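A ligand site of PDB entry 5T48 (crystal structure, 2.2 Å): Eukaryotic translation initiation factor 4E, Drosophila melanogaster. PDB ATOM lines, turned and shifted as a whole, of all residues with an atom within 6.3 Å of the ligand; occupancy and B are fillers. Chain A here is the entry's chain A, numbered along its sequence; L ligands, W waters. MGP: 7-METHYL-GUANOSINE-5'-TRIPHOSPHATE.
O6 of the ligand is in hydrogen-bond range of N of Trp 71.
NH1 of Arg 124 lies within salt-bridge range of O1A of the ligand (3.0 Å).
OE2 of Glu 72 is in hydrogen-bond range of N2 of the ligand, 2.5 Å away.
An oxygen (O2B) of the ligand is in salt-bridge range of the side-chain amino group (NZ) of Lys 129, at 3.5 Å.
An oxygen (O3') of the ligand sits at hydrogen-bond distance from the side-chain amide oxygen of Gln 174 (2.7 Å).
O of Leu 17 sits at hydrogen-bond distance from N of Asp 59 (2.9 Å).
The side-chain carboxylate (OD1) of Asp 59 lies within salt-bridge range of the guanidinium group (NH2) of Arg 124 (3.0 Å).
OD1 of Asp 59 lies within hydrogen-bond range of ND2 of Asn 122 (3.0 Å).
The backbone carbonyl oxygen (O) of Lys 129 sits at hydrogen-bond distance from the backbone NH (N) of Asn 122, 2.6 Å away.
Trp 25 touches the ligand (CZ2 to N7, 3.3 Å).
Asp 59 touches the ligand.
CA of Met 70 touches O6 of the ligand (3.1 Å).
Asn 122 touches the ligand (ND2 to O1A, 3.9 Å).
Water W2 lies within hydrogen-bond range of an oxygen (O2A) of the ligand (2.5 Å) and the guanidinium group of Arg 81 (3.3 Å).
Water W1 lies within hydrogen-bond range of an oxygen (O1B) of the ligand and the guanidinium group of Arg 124.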
ATOM      1  N   LEU A  17      20.960  14.694  16.038  1.00  0.00           N
ATOM      2  CA  LEU A  17      21.612  15.262  17.215  1.00  0.00           C
ATOM      3  C   LEU A  17      22.532  14.215  17.815  1.00  0.00           C
ATOM      4  O   LEU A  17      22.106  13.075  18.035  1.00  0.00           O
ATOM      5  CB  LEU A  17      20.580  15.733  18.240  1.00  0.00           C
ATOM      6  CG  LEU A  17      21.156  16.394  19.498  1.00  0.00           C
ATOM      7  CD1 LEU A  17      20.274  17.557  19.937  1.00  0.00           C
ATOM      8  CD2 LEU A  17      21.299  15.394  20.637  1.00  0.00           C
ATOM      9  N   TRP A  25      23.273  22.791  23.088  1.00  0.00           N
ATOM     10  CA  TRP A  25      22.321  21.809  22.566  1.00  0.00           C
ATOM     11  C   TRP A  25      22.004  22.088  21.101  1.00  0.00           C
ATOM     12  O   TRP A  25      21.953  21.170  20.280  1.00  0.00           O
ATOM     13  CB  TRP A  25      21.045  21.803  23.403  1.00  0.00           C
ATOM     14  CG  TRP A  25      20.035  20.808  22.914  1.00  0.00           C
ATOM     15  CD1 TRP A  25      19.949  19.495  23.266  1.00  0.00           C
ATOM     16  CD2 TRP A  25      18.982  21.052  21.984  1.00  0.00           C
ATOM     17  NE1 TRP A  25      18.897  18.900  22.616  1.00  0.00           N
ATOM     18  CE2 TRP A  25      18.289  19.836  21.818  1.00  0.00           C
ATOM     19  CE3 TRP A  25      18.559  22.171  21.275  1.00  0.00           C
ATOM     20  CZ2 TRP A  25      17.186  19.715  20.973  1.00  0.00           C
ATOM     21  CZ3 TRP A  25      17.465  22.054  20.429  1.00  0.00           C
ATOM     22  CH2 TRP A  25      16.788  20.832  20.291  1.00  0.00           C
ATOM     23  N   GLU A  26      21.759  23.363  20.760  1.00  0.00           N
ATOM     24  CA  GLU A  26      21.488  23.719  19.371  1.00  0.00           C
ATOM     25  C   GLU A  26      22.601  23.241  18.449  1.00  0.00           C
ATOM     26  O   GLU A  26      22.338  22.684  17.373  1.00  0.00           O
ATOM     27  CB  GLU A  26      21.302  25.223  19.242  1.00  0.00           C
ATOM     28  CG  GLU A  26      21.198  25.728  17.803  1.00  0.00           C
ATOM     29  CD  GLU A  26      20.945  27.214  17.708  1.00  0.00           C
ATOM     30  OE1 GLU A  26      21.047  27.900  18.745  1.00  0.00           O
ATOM     31  OE2 GLU A  26      20.659  27.692  16.593  1.00  0.00           O
ATOM     32  N   ASP A  59      19.524  11.962  18.712  1.00  0.00           N
ATOM     33  CA  ASP A  59      18.171  12.098  18.197  1.00  0.00           C
ATOM     34  C   ASP A  59      18.183  12.019  16.676  1.00  0.00           C
ATOM     35  O   ASP A  59      19.168  12.378  16.021  1.00  0.00           O
ATOM     36  CB  ASP A  59      17.528  13.424  18.590  1.00  0.00           C
ATOM     37  CG  ASP A  59      17.570  13.697  20.070  1.00  0.00           C
ATOM     38  OD1 ASP A  59      17.680  12.739  20.866  1.00  0.00           O
ATOM     39  OD2 ASP A  59      17.475  14.878  20.434  1.00  0.00           O
ATOM     40  N   PRO A  69      14.197  21.784  14.749  1.00  0.00           N
ATOM     41  CA  PRO A  69      13.619  20.834  15.727  1.00  0.00           C
ATOM     42  C   PRO A  69      13.836  21.286  17.176  1.00  0.00           C
ATOM     43  O   PRO A  69      14.421  20.571  17.991  1.00  0.00           O
ATOM     44  CB  PRO A  69      14.364  19.541  15.391  1.00  0.00           C
ATOM     45  CG  PRO A  69      15.709  20.007  14.951  1.00  0.00           C
ATOM     46  CD  PRO A  69      15.476  21.296  14.210  1.00  0.00           C
ATOM     47  N   MET A  70      13.337  22.475  17.502  1.00  0.00           N
ATOM     48  CA  MET A  70      13.589  23.034  18.827  1.00  0.00           C
ATOM     49  C   MET A  70      12.429  23.921  19.247  1.00  0.00           C
ATOM     50  O   MET A  70      11.650  24.420  18.417  1.00  0.00           O
ATOM     51  CB  MET A  70      14.900  23.823  18.851  1.00  0.00           C
ATOM     52  CG  MET A  70      15.003  24.909  17.792  1.00  0.00           C
ATOM     53  SD  MET A  70      16.668  25.605  17.693  1.00  0.00           S
ATOM     54  CE  MET A  70      17.609  24.179  17.146  1.00  0.00           C
ATOM     55  N   TRP A  71      12.329  24.133  20.562  1.00  0.00           N
ATOM     56  CA  TRP A  71      11.261  24.957  21.118  1.00  0.00           C
ATOM     57  C   TRP A  71      11.339  26.382  20.585  1.00  0.00           C
ATOM     58  O   TRP A  71      10.305  27.013  20.318  1.00  0.00           O
ATOM     59  CB  TRP A  71      11.347  24.959  22.641  1.00  0.00           C
ATOM     60  CG  TRP A  71      11.398  23.607  23.261  1.00  0.00           C
ATOM     61  CD1 TRP A  71      10.671  22.505  22.902  1.00  0.00           C
ATOM     62  CD2 TRP A  71      12.239  23.188  24.351  1.00  0.00           C
ATOM     63  NE1 TRP A  71      11.001  21.431  23.704  1.00  0.00           N
ATOM     64  CE2 TRP A  71      11.962  21.833  24.603  1.00  0.00           C
ATOM     65  CE3 TRP A  71      13.193  23.844  25.136  1.00  0.00           C
ATOM     66  CZ2 TRP A  71      12.603  21.111  25.601  1.00  0.00           C
ATOM     67  CZ3 TRP A  71      13.833  23.122  26.134  1.00  0.00           C
ATOM     68  CH2 TRP A  71      13.540  21.772  26.358  1.00  0.00           C
ATOM     69  N   GLU A  72      12.554  26.909  20.416  1.00  0.00           N
ATOM     70  CA  GLU A  72      12.722  28.332  20.121  1.00  0.00           C
ATOM     71  C   GLU A  72      12.109  28.703  18.776  1.00  0.00           C
ATOM     72  O   GLU A  72      11.687  29.846  18.583  1.00  0.00           O
ATOM     73  CB  GLU A  72      14.200  28.712  20.130  1.00  0.00           C
ATOM     74  CG  GLU A  72      14.872  28.582  21.494  1.00  0.00           C
ATOM     75  CD  GLU A  72      15.287  27.171  21.810  1.00  0.00           C
ATOM     76  OE1 GLU A  72      14.823  26.243  21.117  1.00  0.00           O
ATOM     77  OE2 GLU A  72      16.090  26.971  22.747  1.00  0.00           O
ATOM     78  N   ARG A  81       3.872  18.432  21.768  1.00  0.00           N
ATOM     79  CA  ARG A  81       4.334  17.198  21.156  1.00  0.00           C
ATOM     80  C   ARG A  81       3.543  16.013  21.695  1.00  0.00           C
ATOM     81  O   ARG A  81       3.261  15.946  22.902  1.00  0.00           O
ATOM     82  CB  ARG A  81       5.831  16.977  21.401  1.00  0.00           C
ATOM     83  CG  ARG A  81       6.223  16.946  22.870  1.00  0.00           C
ATOM     84  CD  ARG A  81       7.670  16.503  23.051  1.00  0.00           C
ATOM     85  NE  ARG A  81       8.049  16.421  24.461  1.00  0.00           N
ATOM     86  CZ  ARG A  81       9.226  15.980  24.897  1.00  0.00           C
ATOM     87  NH1 ARG A  81      10.146  15.580  24.034  1.00  0.00           N
ATOM     88  NH2 ARG A  81       9.479  15.945  26.188  1.00  0.00           N
ATOM     89  N   ASN A 122      14.129  10.017  20.472  1.00  0.00           N
ATOM     90  CA  ASN A 122      15.246  10.102  21.391  1.00  0.00           C
ATOM     91  C   ASN A 122      15.719   8.690  21.718  1.00  0.00           C
ATOM     92  O   ASN A 122      14.946   7.884  22.267  1.00  0.00           O
ATOM     93  CB  ASN A 122      14.846  10.819  22.684  1.00  0.00           C
ATOM     94  CG  ASN A 122      14.177  12.164  22.429  1.00  0.00           C
ATOM     95  OD1 ASN A 122      13.019  12.368  22.802  1.00  0.00           O
ATOM     96  ND2 ASN A 122      14.899  13.074  21.796  1.00  0.00           N
ATOM     97  N   ARG A 124      17.901   6.698  24.123  1.00  0.00           N
ATOM     98  CA  ARG A 124      18.474   6.881  25.451  1.00  0.00           C
ATOM     99  C   ARG A 124      18.690   5.522  26.106  1.00  0.00           C
ATOM    100  O   ARG A 124      18.255   4.485  25.599  1.00  0.00           O
ATOM    101  CB  ARG A 124      17.569   7.755  26.329  1.00  0.00           C
ATOM    102  CG  ARG A 124      17.285   9.132  25.775  1.00  0.00           C
ATOM    103  CD  ARG A 124      18.522  10.019  25.801  1.00  0.00           C
ATOM    104  NE  ARG A 124      18.234  11.387  25.391  1.00  0.00           N
ATOM    105  CZ  ARG A 124      18.208  11.816  24.125  1.00  0.00           C
ATOM    106  NH1 ARG A 124      17.929  13.086  23.865  1.00  0.00           N
ATOM    107  NH2 ARG A 124      18.467  10.987  23.126  1.00  0.00           N
ATOM    108  N   LYS A 126      17.780   4.512  29.478  1.00  0.00           N
ATOM    109  CA  LYS A 126      16.640   4.013  30.238  1.00  0.00           C
ATOM    110  C   LYS A 126      15.508   3.608  29.312  1.00  0.00           C
ATOM    111  O   LYS A 126      15.022   2.465  29.357  1.00  0.00           O
ATOM    112  CB  LYS A 126      16.172   5.069  31.242  1.00  0.00           C
ATOM    113  CG  LYS A 126      17.145   5.301  32.397  1.00  0.00           C
ATOM    114  CD  LYS A 126      16.482   6.062  33.542  1.00  0.00           C
ATOM    115  CE  LYS A 126      16.079   7.474  33.127  1.00  0.00           C
ATOM    116  NZ  LYS A 126      17.247   8.315  32.762  1.00  0.00           N
ATOM    117  N   SER A 127      15.049   4.531  28.472  1.00  0.00           N
ATOM    118  CA  SER A 127      13.935   4.249  27.578  1.00  0.00           C
ATOM    119  C   SER A 127      14.004   5.181  26.378  1.00  0.00           C
ATOM    120  O   SER A 127      14.518   6.299  26.490  1.00  0.00           O
ATOM    121  CB  SER A 127      12.585   4.405  28.291  1.00  0.00           C
ATOM    122  OG  SER A 127      12.373   5.750  28.674  1.00  0.00           O
ATOM    123  N   LYS A 129      12.075   7.269  23.099  1.00  0.00           N
ATOM    124  CA  LYS A 129      10.956   8.214  23.072  1.00  0.00           C
ATOM    125  C   LYS A 129      10.754   8.693  21.647  1.00  0.00           C
ATOM    126  O   LYS A 129      11.725   9.076  20.977  1.00  0.00           O
ATOM    127  CB  LYS A 129      11.245   9.393  24.014  1.00  0.00           C
ATOM    128  CG  LYS A 129      10.085  10.318  24.274  1.00  0.00           C
ATOM    129  CD  LYS A 129      10.280  11.071  25.599  1.00  0.00           C
ATOM    130  CE  LYS A 129      11.632  11.787  25.656  1.00  0.00           C
ATOM    131  NZ  LYS A 129      11.857  12.458  26.958  1.00  0.00           N
ATOM    132  N   TRP A 133       5.746  16.696  16.889  1.00  0.00           N
ATOM    133  CA  TRP A 133       5.560  18.093  17.245  1.00  0.00           C
ATOM    134  C   TRP A 133       4.469  18.705  16.385  1.00  0.00           C
ATOM    135  O   TRP A 133       4.497  18.581  15.158  1.00  0.00           O
ATOM    136  CB  TRP A 133       6.870  18.869  17.071  1.00  0.00           C
ATOM    137  CG  TRP A 133       7.940  18.493  18.054  1.00  0.00           C
ATOM    138  CD1 TRP A 133       8.142  17.273  18.619  1.00  0.00           C
ATOM    139  CD2 TRP A 133       8.941  19.358  18.584  1.00  0.00           C
ATOM    140  NE1 TRP A 133       9.218  17.317  19.473  1.00  0.00           N
ATOM    141  CE2 TRP A 133       9.732  18.589  19.472  1.00  0.00           C
ATOM    142  CE3 TRP A 133       9.252  20.704  18.402  1.00  0.00           C
ATOM    143  CZ2 TRP A 133      10.810  19.120  20.169  1.00  0.00           C
ATOM    144  CZ3 TRP A 133      10.334  21.229  19.092  1.00  0.00           C
ATOM    145  CH2 TRP A 133      11.093  20.450  19.962  1.00  0.00           C
ATOM    146  N   THR A 170       7.232  21.929  29.003  1.00  0.00           N
ATOM    147  CA  THR A 170       8.470  21.154  29.074  1.00  0.00           C
ATOM    148  C   THR A 170       9.709  22.031  28.945  1.00  0.00           C
ATOM    149  O   THR A 170      10.787  21.626  29.375  1.00  0.00           O
ATOM    150  CB  THR A 170       8.491  20.073  27.988  1.00  0.00           C
ATOM    151  OG1 THR A 170       9.698  19.314  28.073  1.00  0.00           O
ATOM    152  CG2 THR A 170       8.375  20.696  26.603  1.00  0.00           C
ATOM    153  N   LYS A 173      10.450  23.196  32.687  1.00  0.00           N
ATOM    154  CA  LYS A 173      10.875  22.131  33.598  1.00  0.00           C
ATOM    155  C   LYS A 173      12.009  21.360  32.942  1.00  0.00           C
ATOM    156  O   LYS A 173      11.782  20.529  32.059  1.00  0.00           O
ATOM    157  CB  LYS A 173       9.694  21.224  33.933  1.00  0.00           C
ATOM    158  CG  LYS A 173       8.458  21.987  34.417  1.00  0.00           C
ATOM    159  CD  LYS A 173       8.759  22.806  35.660  1.00  0.00           C
ATOM    160  CE  LYS A 173       7.556  23.647  36.079  1.00  0.00           C
ATOM    161  NZ  LYS A 173       7.901  24.592  37.167  1.00  0.00           N
ATOM    162  N   GLN A 174      13.239  21.619  33.385  1.00  0.00           N
ATOM    163  CA  GLN A 174      14.409  20.970  32.830  1.00  0.00           C
ATOM    164  C   GLN A 174      14.706  19.666  33.569  1.00  0.00           C
ATOM    165  O   GLN A 174      15.788  19.108  33.437  1.00  0.00           O
ATOM    166  CB  GLN A 174      15.626  21.905  32.917  1.00  0.00           C
ATOM    167  CG  GLN A 174      15.402  23.261  32.277  1.00  0.00           C
ATOM    168  CD  GLN A 174      15.176  23.186  30.781  1.00  0.00           C
ATOM    169  OE1 GLN A 174      15.495  22.178  30.143  1.00  0.00           O
ATOM    170  NE2 GLN A 174      14.617  24.242  30.212  1.00  0.00           N
ATOM    171  N   ASN A 177       8.038  14.807  35.843  1.00  0.00           N
ATOM    172  CA  ASN A 177       8.467  16.191  36.050  1.00  0.00           C
ATOM    173  C   ASN A 177       7.675  17.160  35.166  1.00  0.00           C
ATOM    174  O   ASN A 177       7.678  18.369  35.409  1.00  0.00           O
ATOM    175  CB  ASN A 177       9.963  16.330  35.760  1.00  0.00           C
ATOM    176  CG  ASN A 177      10.416  17.775  35.718  1.00  0.00           C
ATOM    177  OD1 ASN A 177      10.729  18.307  34.648  1.00  0.00           O
ATOM    178  ND2 ASN A 177      10.451  18.417  36.876  1.00  0.00           N
ATOM    179  N   VAL A 178       6.988  16.625  34.166  1.00  0.00           N
ATOM    180  CA  VAL A 178       6.342  17.437  33.132  1.00  0.00           C
ATOM    181  C   VAL A 178       4.912  16.936  32.954  1.00  0.00           C
ATOM    182  O   VAL A 178       4.686  15.734  32.785  1.00  0.00           O
ATOM    183  CB  VAL A 178       7.119  17.357  31.801  1.00  0.00           C
ATOM    184  CG1 VAL A 178       6.435  18.171  30.719  1.00  0.00           C
ATOM    185  CG2 VAL A 178       8.555  17.855  32.014  1.00  0.00           C
HETATM  186  PA  MGP L   1      15.931  15.698  25.426  1.00  0.00           P
HETATM  187  O1A MGP L   1      16.605  15.746  24.068  1.00  0.00           O
HETATM  188  O2A MGP L   1      14.550  16.219  25.299  1.00  0.00           O
HETATM  189  O3A MGP L   1      15.894  14.189  25.929  1.00  0.00           O
HETATM  190  O5' MGP L   1      16.855  16.522  26.461  1.00  0.00           O
HETATM  191  PB  MGP L   1      15.924  13.525  27.378  1.00  0.00           P
HETATM  192  O1B MGP L   1      17.366  13.499  27.879  1.00  0.00           O
HETATM  193  O2B MGP L   1      15.373  12.166  27.331  1.00  0.00           O
HETATM  194  O3B MGP L   1      15.066  14.438  28.371  1.00  0.00           O
HETATM  195  PC  MGP L   1      14.748  14.285  29.920  1.00  0.00           P
HETATM  196  O1C MGP L   1      16.074  13.994  30.613  1.00  0.00           O
HETATM  197  O2C MGP L   1      14.093  15.524  30.427  1.00  0.00           O
HETATM  198  O3C MGP L   1      13.866  13.052  30.063  1.00  0.00           O
HETATM  199  C5' MGP L   1      16.304  17.593  27.262  1.00  0.00           C
HETATM  200  C4' MGP L   1      17.365  18.652  27.452  1.00  0.00           C
HETATM  201  O4' MGP L   1      17.981  18.956  26.180  1.00  0.00           O
HETATM  202  C3' MGP L   1      16.838  19.978  28.002  1.00  0.00           C
HETATM  203  O3' MGP L   1      16.997  20.012  29.405  1.00  0.00           O
HETATM  204  C2' MGP L   1      17.710  21.018  27.286  1.00  0.00           C
HETATM  205  O2' MGP L   1      18.940  21.236  27.968  1.00  0.00           O
HETATM  206  C1' MGP L   1      17.945  20.347  25.933  1.00  0.00           C
HETATM  207  N9  MGP L   1      16.888  20.609  24.939  1.00  0.00           N
HETATM  208  C8  MGP L   1      16.028  19.703  24.484  1.00  0.00           C
HETATM  209  N7  MGP L   1      15.239  20.273  23.591  1.00  0.00           N
HETATM  210  CM7 MGP L   1      14.166  19.574  22.859  1.00  0.00           C
HETATM  211  C5  MGP L   1      15.584  21.608  23.466  1.00  0.00           C
HETATM  212  C6  MGP L   1      15.085  22.682  22.679  1.00  0.00           C
HETATM  213  O6  MGP L   1      14.155  22.670  21.872  1.00  0.00           O
HETATM  214  N1  MGP L   1      15.794  23.840  22.927  1.00  0.00           N
HETATM  215  C2  MGP L   1      16.841  23.966  23.804  1.00  0.00           C
HETATM  216  N2  MGP L   1      17.399  25.171  23.906  1.00  0.00           N
HETATM  217  N3  MGP L   1      17.301  22.956  24.537  1.00  0.00           N
HETATM  218  C4  MGP L   1      16.636  21.808  24.328  1.00  0.00           C
HETATM  219  O   HOH W   1      20.327  13.543  26.878  1.00  0.00           O
HETATM  220  O   HOH W   2      12.485  17.310  26.250  1.00  0.00           O
